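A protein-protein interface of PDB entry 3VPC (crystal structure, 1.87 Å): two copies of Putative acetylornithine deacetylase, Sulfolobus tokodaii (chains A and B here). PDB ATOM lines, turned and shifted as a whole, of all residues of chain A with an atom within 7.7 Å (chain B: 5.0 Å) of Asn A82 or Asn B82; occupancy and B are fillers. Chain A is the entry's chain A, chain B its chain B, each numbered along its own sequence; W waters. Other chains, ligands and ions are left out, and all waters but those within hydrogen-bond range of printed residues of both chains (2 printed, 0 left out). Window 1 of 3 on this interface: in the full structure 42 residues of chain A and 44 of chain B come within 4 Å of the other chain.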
ATOM      1  N   MET A  57      14.839  28.229  15.503  1.00  0.00           N
ATOM      2  CA  MET A  57      16.236  28.612  15.714  1.00  0.00           C
ATOM      3  C   MET A  57      16.462  30.113  15.595  1.00  0.00           C
ATOM      4  O   MET A  57      17.079  30.706  16.474  1.00  0.00           O
ATOM      5  CB  MET A  57      17.200  27.827  14.809  1.00  0.00           C
ATOM      6  CG  MET A  57      18.682  28.208  15.058  1.00  0.00           C
ATOM      7  SD  MET A  57      19.827  27.268  14.036  1.00  0.00           S
ATOM      8  CE  MET A  57      21.369  28.101  14.446  1.00  0.00           C
ATOM      9  N   LEU A  61      18.015  32.332  18.477  1.00  0.00           N
ATOM     10  CA  LEU A  61      19.280  32.994  18.218  1.00  0.00           C
ATOM     11  C   LEU A  61      19.172  34.502  18.440  1.00  0.00           C
ATOM     12  O   LEU A  61      20.028  35.113  19.114  1.00  0.00           O
ATOM     13  CB  LEU A  61      19.764  32.682  16.783  1.00  0.00           C
ATOM     14  CG  LEU A  61      21.074  33.363  16.336  1.00  0.00           C
ATOM     15  CD1 LEU A  61      22.289  32.902  17.121  1.00  0.00           C
ATOM     16  CD2 LEU A  61      21.305  33.103  14.844  1.00  0.00           C
ATOM     17  N   TYR A  62      18.138  35.107  17.858  1.00  0.00           N
ATOM     18  CA  TYR A  62      18.055  36.558  17.865  1.00  0.00           C
ATOM     19  C   TYR A  62      17.586  37.117  19.196  1.00  0.00           C
ATOM     20  O   TYR A  62      18.029  38.173  19.589  1.00  0.00           O
ATOM     21  CB  TYR A  62      17.197  37.065  16.707  1.00  0.00           C
ATOM     22  CG  TYR A  62      17.788  36.766  15.344  1.00  0.00           C
ATOM     23  CD1 TYR A  62      16.966  36.402  14.280  1.00  0.00           C
ATOM     24  CD2 TYR A  62      19.177  36.845  15.127  1.00  0.00           C
ATOM     25  CE1 TYR A  62      17.503  36.120  13.021  1.00  0.00           C
ATOM     26  CE2 TYR A  62      19.715  36.584  13.897  1.00  0.00           C
ATOM     27  CZ  TYR A  62      18.874  36.217  12.844  1.00  0.00           C
ATOM     28  OH  TYR A  62      19.379  35.955  11.604  1.00  0.00           O
ATOM     29  N   SER A  77      23.573  30.594  25.239  1.00  0.00           N
ATOM     30  CA  SER A  77      24.077  31.827  24.629  1.00  0.00           C
ATOM     31  C   SER A  77      23.994  31.786  23.090  1.00  0.00           C
ATOM     32  O   SER A  77      23.907  30.688  22.512  1.00  0.00           O
ATOM     33  CB  SER A  77      25.525  32.068  25.081  1.00  0.00           C
ATOM     34  OG  SER A  77      26.397  31.255  24.331  1.00  0.00           O
ATOM     35  N   SER A  78      24.071  32.963  22.445  1.00  0.00           N
ATOM     36  CA  SER A  78      23.888  33.070  20.982  1.00  0.00           C
ATOM     37  C   SER A  78      24.942  32.273  20.204  1.00  0.00           C
ATOM     38  O   SER A  78      24.632  31.666  19.173  1.00  0.00           O
ATOM     39  CB  SER A  78      23.837  34.529  20.507  1.00  0.00           C
ATOM     40  OG  SER A  78      25.066  35.206  20.787  1.00  0.00           O
ATOM     41  N   ASP A  79      26.176  32.264  20.705  1.00  0.00           N
ATOM     42  CA  ASP A  79      27.249  31.515  20.047  1.00  0.00           C
ATOM     43  C   ASP A  79      26.969  30.019  20.145  1.00  0.00           C
ATOM     44  O   ASP A  79      27.151  29.291  19.179  1.00  0.00           O
ATOM     45  CB  ASP A  79      28.628  31.880  20.614  1.00  0.00           C
ATOM     46  CG  ASP A  79      28.742  31.612  22.100  1.00  0.00           C
ATOM     47  OD1 ASP A  79      27.905  32.142  22.855  1.00  0.00           O
ATOM     48  OD2 ASP A  79      29.658  30.869  22.511  1.00  0.00           O
ATOM     49  N   VAL A  80      26.479  29.584  21.306  1.00  0.00           N
ATOM     50  CA  VAL A  80      26.132  28.178  21.547  1.00  0.00           C
ATOM     51  C   VAL A  80      24.951  27.758  20.667  1.00  0.00           C
ATOM     52  O   VAL A  80      24.953  26.672  20.104  1.00  0.00           O
ATOM     53  CB  VAL A  80      25.865  27.916  23.060  1.00  0.00           C
ATOM     54  CG1 VAL A  80      25.218  26.537  23.293  1.00  0.00           C
ATOM     55  CG2 VAL A  80      27.176  28.065  23.866  1.00  0.00           C
ATOM     56  N   ILE A  81      23.962  28.629  20.523  1.00  0.00           N
ATOM     57  CA  ILE A  81      22.827  28.363  19.629  1.00  0.00           C
ATOM     58  C   ILE A  81      23.297  28.232  18.176  1.00  0.00           C
ATOM     59  O   ILE A  81      22.840  27.363  17.452  1.00  0.00           O
ATOM     60  CB  ILE A  81      21.720  29.447  19.765  1.00  0.00           C
ATOM     61  CG1 ILE A  81      21.035  29.309  21.126  1.00  0.00           C
ATOM     62  CG2 ILE A  81      20.671  29.376  18.629  1.00  0.00           C
ATOM     63  CD1 ILE A  81      20.418  30.592  21.687  1.00  0.00           C
ATOM     64  N   ASN A  82      24.197  29.115  17.763  1.00  0.00           N
ATOM     65  CA  ASN A  82      24.727  29.068  16.405  1.00  0.00           C
ATOM     66  C   ASN A  82      25.507  27.777  16.108  1.00  0.00           C
ATOM     67  O   ASN A  82      25.392  27.225  15.024  1.00  0.00           O
ATOM     68  CB  ASN A  82      25.566  30.319  16.120  1.00  0.00           C
ATOM     69  CG  ASN A  82      24.915  31.253  15.097  1.00  0.00           C
ATOM     70  OD1 ASN A  82      25.206  32.458  15.072  1.00  0.00           O
ATOM     71  ND2 ASN A  82      24.048  30.706  14.231  1.00  0.00           N
ATOM     72  N   VAL A  83      26.274  27.299  17.086  1.00  0.00           N
ATOM     73  CA  VAL A  83      27.033  26.058  16.955  1.00  0.00           C
ATOM     74  C   VAL A  83      26.132  24.817  17.023  1.00  0.00           C
ATOM     75  O   VAL A  83      26.194  23.966  16.133  1.00  0.00           O
ATOM     76  CB  VAL A  83      28.193  25.984  17.978  1.00  0.00           C
ATOM     77  CG1 VAL A  83      28.875  24.623  17.960  1.00  0.00           C
ATOM     78  CG2 VAL A  83      29.227  27.076  17.686  1.00  0.00           C
ATOM     79  N   CYS A  84      25.307  24.700  18.073  1.00  0.00           N
ATOM     80  CA  CYS A  84      24.448  23.520  18.223  1.00  0.00           C
ATOM     81  C   CYS A  84      23.441  23.394  17.080  1.00  0.00           C
ATOM     82  O   CYS A  84      23.151  22.276  16.613  1.00  0.00           O
ATOM     83  CB  CYS A  84      23.715  23.563  19.567  1.00  0.00           C
ATOM     84  SG  CYS A  84      24.826  23.353  20.934  1.00  0.00           S
ATOM     85  N   GLY A  85      22.916  24.538  16.627  1.00  0.00           N
ATOM     86  CA  GLY A  85      21.914  24.573  15.585  1.00  0.00           C
ATOM     87  C   GLY A  85      22.436  24.192  14.200  1.00  0.00           C
ATOM     88  O   GLY A  85      21.659  24.046  13.261  1.00  0.00           O
ATOM     89  N   ASP A  86      23.746  24.007  14.082  1.00  0.00           N
ATOM     90  CA  ASP A  86      24.347  23.663  12.797  1.00  0.00           C
ATOM     91  C   ASP A  86      25.295  22.493  12.946  1.00  0.00           C
ATOM     92  O   ASP A  86      26.339  22.634  13.567  1.00  0.00           O
ATOM     93  CB  ASP A  86      25.135  24.855  12.248  1.00  0.00           C
ATOM     94  CG  ASP A  86      25.484  24.671  10.789  1.00  0.00           C
ATOM     95  OD1 ASP A  86      24.887  25.348   9.957  1.00  0.00           O
ATOM     96  OD2 ASP A  86      26.303  23.798  10.475  1.00  0.00           O
ATOM     97  N   LYS A  87      24.972  21.364  12.314  1.00  0.00           N
ATOM     98  CA  LYS A  87      25.763  20.177  12.525  1.00  0.00           C
ATOM     99  C   LYS A  87      27.175  20.296  12.014  1.00  0.00           C
ATOM    100  O   LYS A  87      28.031  19.690  12.584  1.00  0.00           O
ATOM    101  CB  LYS A  87      25.104  18.916  11.919  1.00  0.00           C
ATOM    102  CG  LYS A  87      23.716  18.568  12.527  1.00  0.00           C
ATOM    103  CD  LYS A  87      23.065  17.471  11.666  1.00  0.00           C
ATOM    104  CE  LYS A  87      21.687  17.107  12.135  1.00  0.00           C
ATOM    105  NZ  LYS A  87      21.926  16.023  13.116  1.00  0.00           N
ATOM    106  N   ILE A  88      27.411  21.043  10.932  1.00  0.00           N
ATOM    107  CA  ILE A  88      28.789  21.245  10.468  1.00  0.00           C
ATOM    108  C   ILE A  88      29.633  21.973  11.527  1.00  0.00           C
ATOM    109  O   ILE A  88      30.756  21.570  11.822  1.00  0.00           O
ATOM    110  CB  ILE A  88      28.861  21.965   9.078  1.00  0.00           C
ATOM    111  CG1 ILE A  88      28.315  21.039   7.991  1.00  0.00           C
ATOM    112  CG2 ILE A  88      30.294  22.386   8.786  1.00  0.00           C
ATOM    113  CD1 ILE A  88      28.047  21.701   6.622  1.00  0.00           C
ATOM    114  N   LEU A  89      29.087  23.039  12.083  1.00  0.00           N
ATOM    115  CA  LEU A  89      29.771  23.780  13.143  1.00  0.00           C
ATOM    116  C   LEU A  89      29.974  22.925  14.396  1.00  0.00           C
ATOM    117  O   LEU A  89      31.051  22.921  14.979  1.00  0.00           O
ATOM    118  CB  LEU A  89      29.009  25.057  13.453  1.00  0.00           C
ATOM    119  CG  LEU A  89      28.746  26.036  12.302  1.00  0.00           C
ATOM    120  CD1 LEU A  89      28.069  27.270  12.833  1.00  0.00           C
ATOM    121  CD2 LEU A  89      30.049  26.422  11.555  1.00  0.00           C
ATOM    122  N   THR A  90      28.937  22.189  14.797  1.00  0.00           N
ATOM    123  CA  THR A  90      29.073  21.195  15.881  1.00  0.00           C
ATOM    124  C   THR A  90      30.188  20.144  15.611  1.00  0.00           C
ATOM    125  O   THR A  90      31.087  19.953  16.448  1.00  0.00           O
ATOM    126  CB  THR A  90      27.751  20.501  16.146  1.00  0.00           C
ATOM    127  OG1 THR A  90      26.861  21.429  16.792  1.00  0.00           O
ATOM    128  CG2 THR A  90      27.966  19.301  17.060  1.00  0.00           C
ATOM    129  N   ILE A 130      21.238  21.596   8.877  1.00  0.00           N
ATOM    130  CA  ILE A 130      20.175  22.234   9.642  1.00  0.00           C
ATOM    131  C   ILE A 130      19.043  21.234   9.905  1.00  0.00           C
ATOM    132  O   ILE A 130      18.641  20.488   9.011  1.00  0.00           O
ATOM    133  CB  ILE A 130      19.702  23.554   8.919  1.00  0.00           C
ATOM    134  CG1 ILE A 130      20.329  24.788   9.570  1.00  0.00           C
ATOM    135  CG2 ILE A 130      18.194  23.688   8.899  1.00  0.00           C
ATOM    136  CD1 ILE A 130      21.826  25.001   9.290  1.00  0.00           C
ATOM    137  N   ASP A 253      20.175  22.950  21.225  1.00  0.00           N
ATOM    138  CA  ASP A 253      20.263  24.089  22.158  1.00  0.00           C
ATOM    139  C   ASP A 253      18.920  24.516  22.775  1.00  0.00           C
ATOM    140  O   ASP A 253      18.885  25.285  23.738  1.00  0.00           O
ATOM    141  CB  ASP A 253      20.934  25.267  21.470  1.00  0.00           C
ATOM    142  CG  ASP A 253      20.191  25.696  20.234  1.00  0.00           C
ATOM    143  OD1 ASP A 253      19.273  26.534  20.352  1.00  0.00           O
ATOM    144  OD2 ASP A 253      20.510  25.184  19.155  1.00  0.00           O
ATOM    145  N   LEU B  61      31.352  30.046   5.660  1.00  0.00           N
ATOM    146  CA  LEU B  61      31.181  29.534   7.005  1.00  0.00           C
ATOM    147  C   LEU B  61      31.666  28.085   7.131  1.00  0.00           C
ATOM    148  O   LEU B  61      32.441  27.730   8.057  1.00  0.00           O
ATOM    149  CB  LEU B  61      29.715  29.638   7.431  1.00  0.00           C
ATOM    150  CG  LEU B  61      29.337  29.131   8.827  1.00  0.00           C
ATOM    151  CD1 LEU B  61      29.967  30.006   9.902  1.00  0.00           C
ATOM    152  CD2 LEU B  61      27.833  29.148   8.995  1.00  0.00           C
ATOM    153  N   SER B  78      35.266  30.824  11.507  1.00  0.00           N
ATOM    154  CA  SER B  78      33.848  30.519  11.338  1.00  0.00           C
ATOM    155  C   SER B  78      32.980  31.270  12.347  1.00  0.00           C
ATOM    156  O   SER B  78      31.879  31.705  12.014  1.00  0.00           O
ATOM    157  CB  SER B  78      33.566  28.997  11.360  1.00  0.00           C
ATOM    158  OG  SER B  78      33.782  28.451  12.633  1.00  0.00           O
ATOM    159  N   ASP B  79      33.471  31.413  13.571  1.00  0.00           N
ATOM    160  CA  ASP B  79      32.762  32.175  14.599  1.00  0.00           C
ATOM    161  C   ASP B  79      32.523  33.615  14.101  1.00  0.00           C
ATOM    162  O   ASP B  79      31.421  34.145  14.228  1.00  0.00           O
ATOM    163  CB  ASP B  79      33.534  32.137  15.942  1.00  0.00           C
ATOM    164  CG  ASP B  79      33.731  30.693  16.491  1.00  0.00           C
ATOM    165  OD1 ASP B  79      34.705  30.445  17.252  1.00  0.00           O
ATOM    166  OD2 ASP B  79      32.921  29.789  16.169  1.00  0.00           O
ATOM    167  N   VAL B  80      33.552  34.208  13.488  1.00  0.00           N
ATOM    168  CA  VAL B  80      33.544  35.609  13.026  1.00  0.00           C
ATOM    169  C   VAL B  80      32.635  35.779  11.811  1.00  0.00           C
ATOM    170  O   VAL B  80      31.917  36.782  11.688  1.00  0.00           O
ATOM    171  CB  VAL B  80      35.009  36.120  12.767  1.00  0.00           C
ATOM    172  CG1 VAL B  80      35.035  37.443  11.975  1.00  0.00           C
ATOM    173  CG2 VAL B  80      35.753  36.284  14.095  1.00  0.00           C
ATOM    174  N   ILE B  81      32.660  34.785  10.931  1.00  0.00           N
ATOM    175  CA  ILE B  81      31.774  34.766   9.778  1.00  0.00           C
ATOM    176  C   ILE B  81      30.318  34.692  10.204  1.00  0.00           C
ATOM    177  O   ILE B  81      29.494  35.415   9.656  1.00  0.00           O
ATOM    178  CB  ILE B  81      32.092  33.613   8.808  1.00  0.00           C
ATOM    179  CG1 ILE B  81      33.398  33.911   8.086  1.00  0.00           C
ATOM    180  CG2 ILE B  81      30.945  33.403   7.802  1.00  0.00           C
ATOM    181  CD1 ILE B  81      34.102  32.631   7.567  1.00  0.00           C
ATOM    182  N   ASN B  82      30.012  33.843  11.180  1.00  0.00           N
ATOM    183  CA  ASN B  82      28.632  33.761  11.730  1.00  0.00           C
ATOM    184  C   ASN B  82      28.145  35.117  12.263  1.00  0.00           C
ATOM    185  O   ASN B  82      27.039  35.550  11.973  1.00  0.00           O
ATOM    186  CB  ASN B  82      28.518  32.666  12.808  1.00  0.00           C
ATOM    187  CG  ASN B  82      27.559  31.505  12.402  1.00  0.00           C
ATOM    188  OD1 ASN B  82      27.699  30.384  12.899  1.00  0.00           O
ATOM    189  ND2 ASN B  82      26.596  31.775  11.513  1.00  0.00           N
ATOM    190  N   VAL B  83      29.017  35.818  12.973  1.00  0.00           N
ATOM    191  CA  VAL B  83      28.688  37.138  13.521  1.00  0.00           C
ATOM    192  C   VAL B  83      28.582  38.242  12.466  1.00  0.00           C
ATOM    193  O   VAL B  83      27.540  38.885  12.361  1.00  0.00           O
ATOM    194  CB  VAL B  83      29.655  37.514  14.668  1.00  0.00           C
ATOM    195  CG1 VAL B  83      29.423  38.968  15.137  1.00  0.00           C
ATOM    196  CG2 VAL B  83      29.467  36.538  15.832  1.00  0.00           C
ATOM    197  N   CYS B  84      29.651  38.451  11.689  1.00  0.00           N
ATOM    198  CA  CYS B  84      29.685  39.445  10.613  1.00  0.00           C
ATOM    199  C   CYS B  84      28.607  39.258   9.547  1.00  0.00           C
ATOM    200  O   CYS B  84      28.040  40.236   9.030  1.00  0.00           O
ATOM    201  CB  CYS B  84      31.076  39.466   9.949  1.00  0.00           C
ATOM    202  SG  CYS B  84      32.335  40.113  11.036  1.00  0.00           S
ATOM    203  N   GLY B  85      28.290  37.996   9.250  1.00  0.00           N
ATOM    204  CA  GLY B  85      27.328  37.694   8.205  1.00  0.00           C
ATOM    205  C   GLY B  85      25.900  37.952   8.637  1.00  0.00           C
ATOM    206  O   GLY B  85      24.986  37.893   7.819  1.00  0.00           O
ATOM    207  N   ASP B  86      25.712  38.258   9.922  1.00  0.00           N
ATOM    208  CA  ASP B  86      24.366  38.488  10.466  1.00  0.00           C
ATOM    209  C   ASP B  86      24.268  39.832  11.170  1.00  0.00           C
ATOM    210  O   ASP B  86      24.958  40.074  12.154  1.00  0.00           O
ATOM    211  CB  ASP B  86      23.970  37.366  11.432  1.00  0.00           C
ATOM    212  CG  ASP B  86      22.514  37.422  11.792  1.00  0.00           C
ATOM    213  OD1 ASP B  86      21.760  36.524  11.355  1.00  0.00           O
ATOM    214  OD2 ASP B  86      22.121  38.363  12.509  1.00  0.00           O
ATOM    215  N   LEU B  89      23.377  39.815  15.103  1.00  0.00           N
ATOM    216  CA  LEU B  89      24.519  39.377  15.905  1.00  0.00           C
ATOM    217  C   LEU B  89      25.594  40.453  15.998  1.00  0.00           C
ATOM    218  O   LEU B  89      26.162  40.690  17.078  1.00  0.00           O
ATOM    219  CB  LEU B  89      25.090  38.068  15.345  1.00  0.00           C
ATOM    220  CG  LEU B  89      24.114  36.890  15.271  1.00  0.00           C
ATOM    221  CD1 LEU B  89      24.875  35.613  14.968  1.00  0.00           C
ATOM    222  CD2 LEU B  89      23.294  36.708  16.576  1.00  0.00           C
HETATM  223  O   HOH W   1      24.935  33.791  12.157  1.00  0.00           O
HETATM  224  O   HOH W   2      24.973  28.563  12.819  1.00  0.00           O
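The side-chain hydroxyl (OH) of Tyr A62 is in hydrogen-bond range of the side-chain carboxylate (OD1) of Asp B86 (2.5 Å).
Of the printed residues of chain B, Tyr A62 touches Asp B86 (2.5 Å). Of chain B, only Asn B82 (3.7 Å) and Leu B89 (3.2 Å) come within 4 Å of Asn A82. Of the printed residues of chain B, Leu A89 touches Leu B61 (3.9 Å) and Asn B82 (3.1 Å). Thr A90 touches none of the printed residues of chain B. Of chain A, only Asn A82 and Leu A89 come within 4 Å of Asn B82. Of the printed residues of chain A, Asp B86 touches Tyr A62 (2.5 Å). Of the printed residues of chain A, Leu B89 touches Leu A61 and Asn A82. The nearest printed residue of chain A that does not touch Leu B89 is Tyr A62 (4.4 Å).
The side-chain carboxylate (OD2) of Asp B86 sits at hydrogen-bond distance from the backbone NH (N) of Leu B89, 3.2 Å away. N of Leu A89 sits at hydrogen-bond distance from OD2 of Asp A86 (3.3 Å).
Among the printed residues, merely in contact across the chains: Leu A61 with Leu B89, Asn A82 with Asn B82, Asn A82 with Leu B89, Leu A89 with Leu B61 and Leu A89 with Asn B82.
Leu A61 touches Leu B89, and with the chains exchanged Leu A89 touches Leu B61. Asn B82 touches its own counterpart, Asn A82. Asn A82 touches Leu B89, and with the chains exchanged Leu A89 touches Asn B82. 11 positions are printed for both chains. Of the 6 pairs that touch across the chains among the printed residues, 5 have their exchanged pair printed and touching as well.
Water W2 lies within hydrogen-bond range of O of Asn A82 (2.6 Å) and OD1 of Asn B82 (3.3 Å). Water W1 lies within hydrogen-bond range of the side-chain amide nitrogen of Asn B82 and the side-chain amide oxygen of Asn A82.
Printed residues of chain B that touch a printed residue of chain A: Leu B61, Asn B82, Asp B86 and Leu B89. Hydrophobic or aromatic side chains of chain B that line the printed part of chain A: Leu B61 and Leu B89. Of the 19 printed residues of chain A, 4 touch a printed residue of chain B. Hydrophobic or aromatic side chains of chain A that line the printed part of chain B: Leu A61, Tyr A62 and Leu A89. Among the printed residues, 6 pairs touch across the chains.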
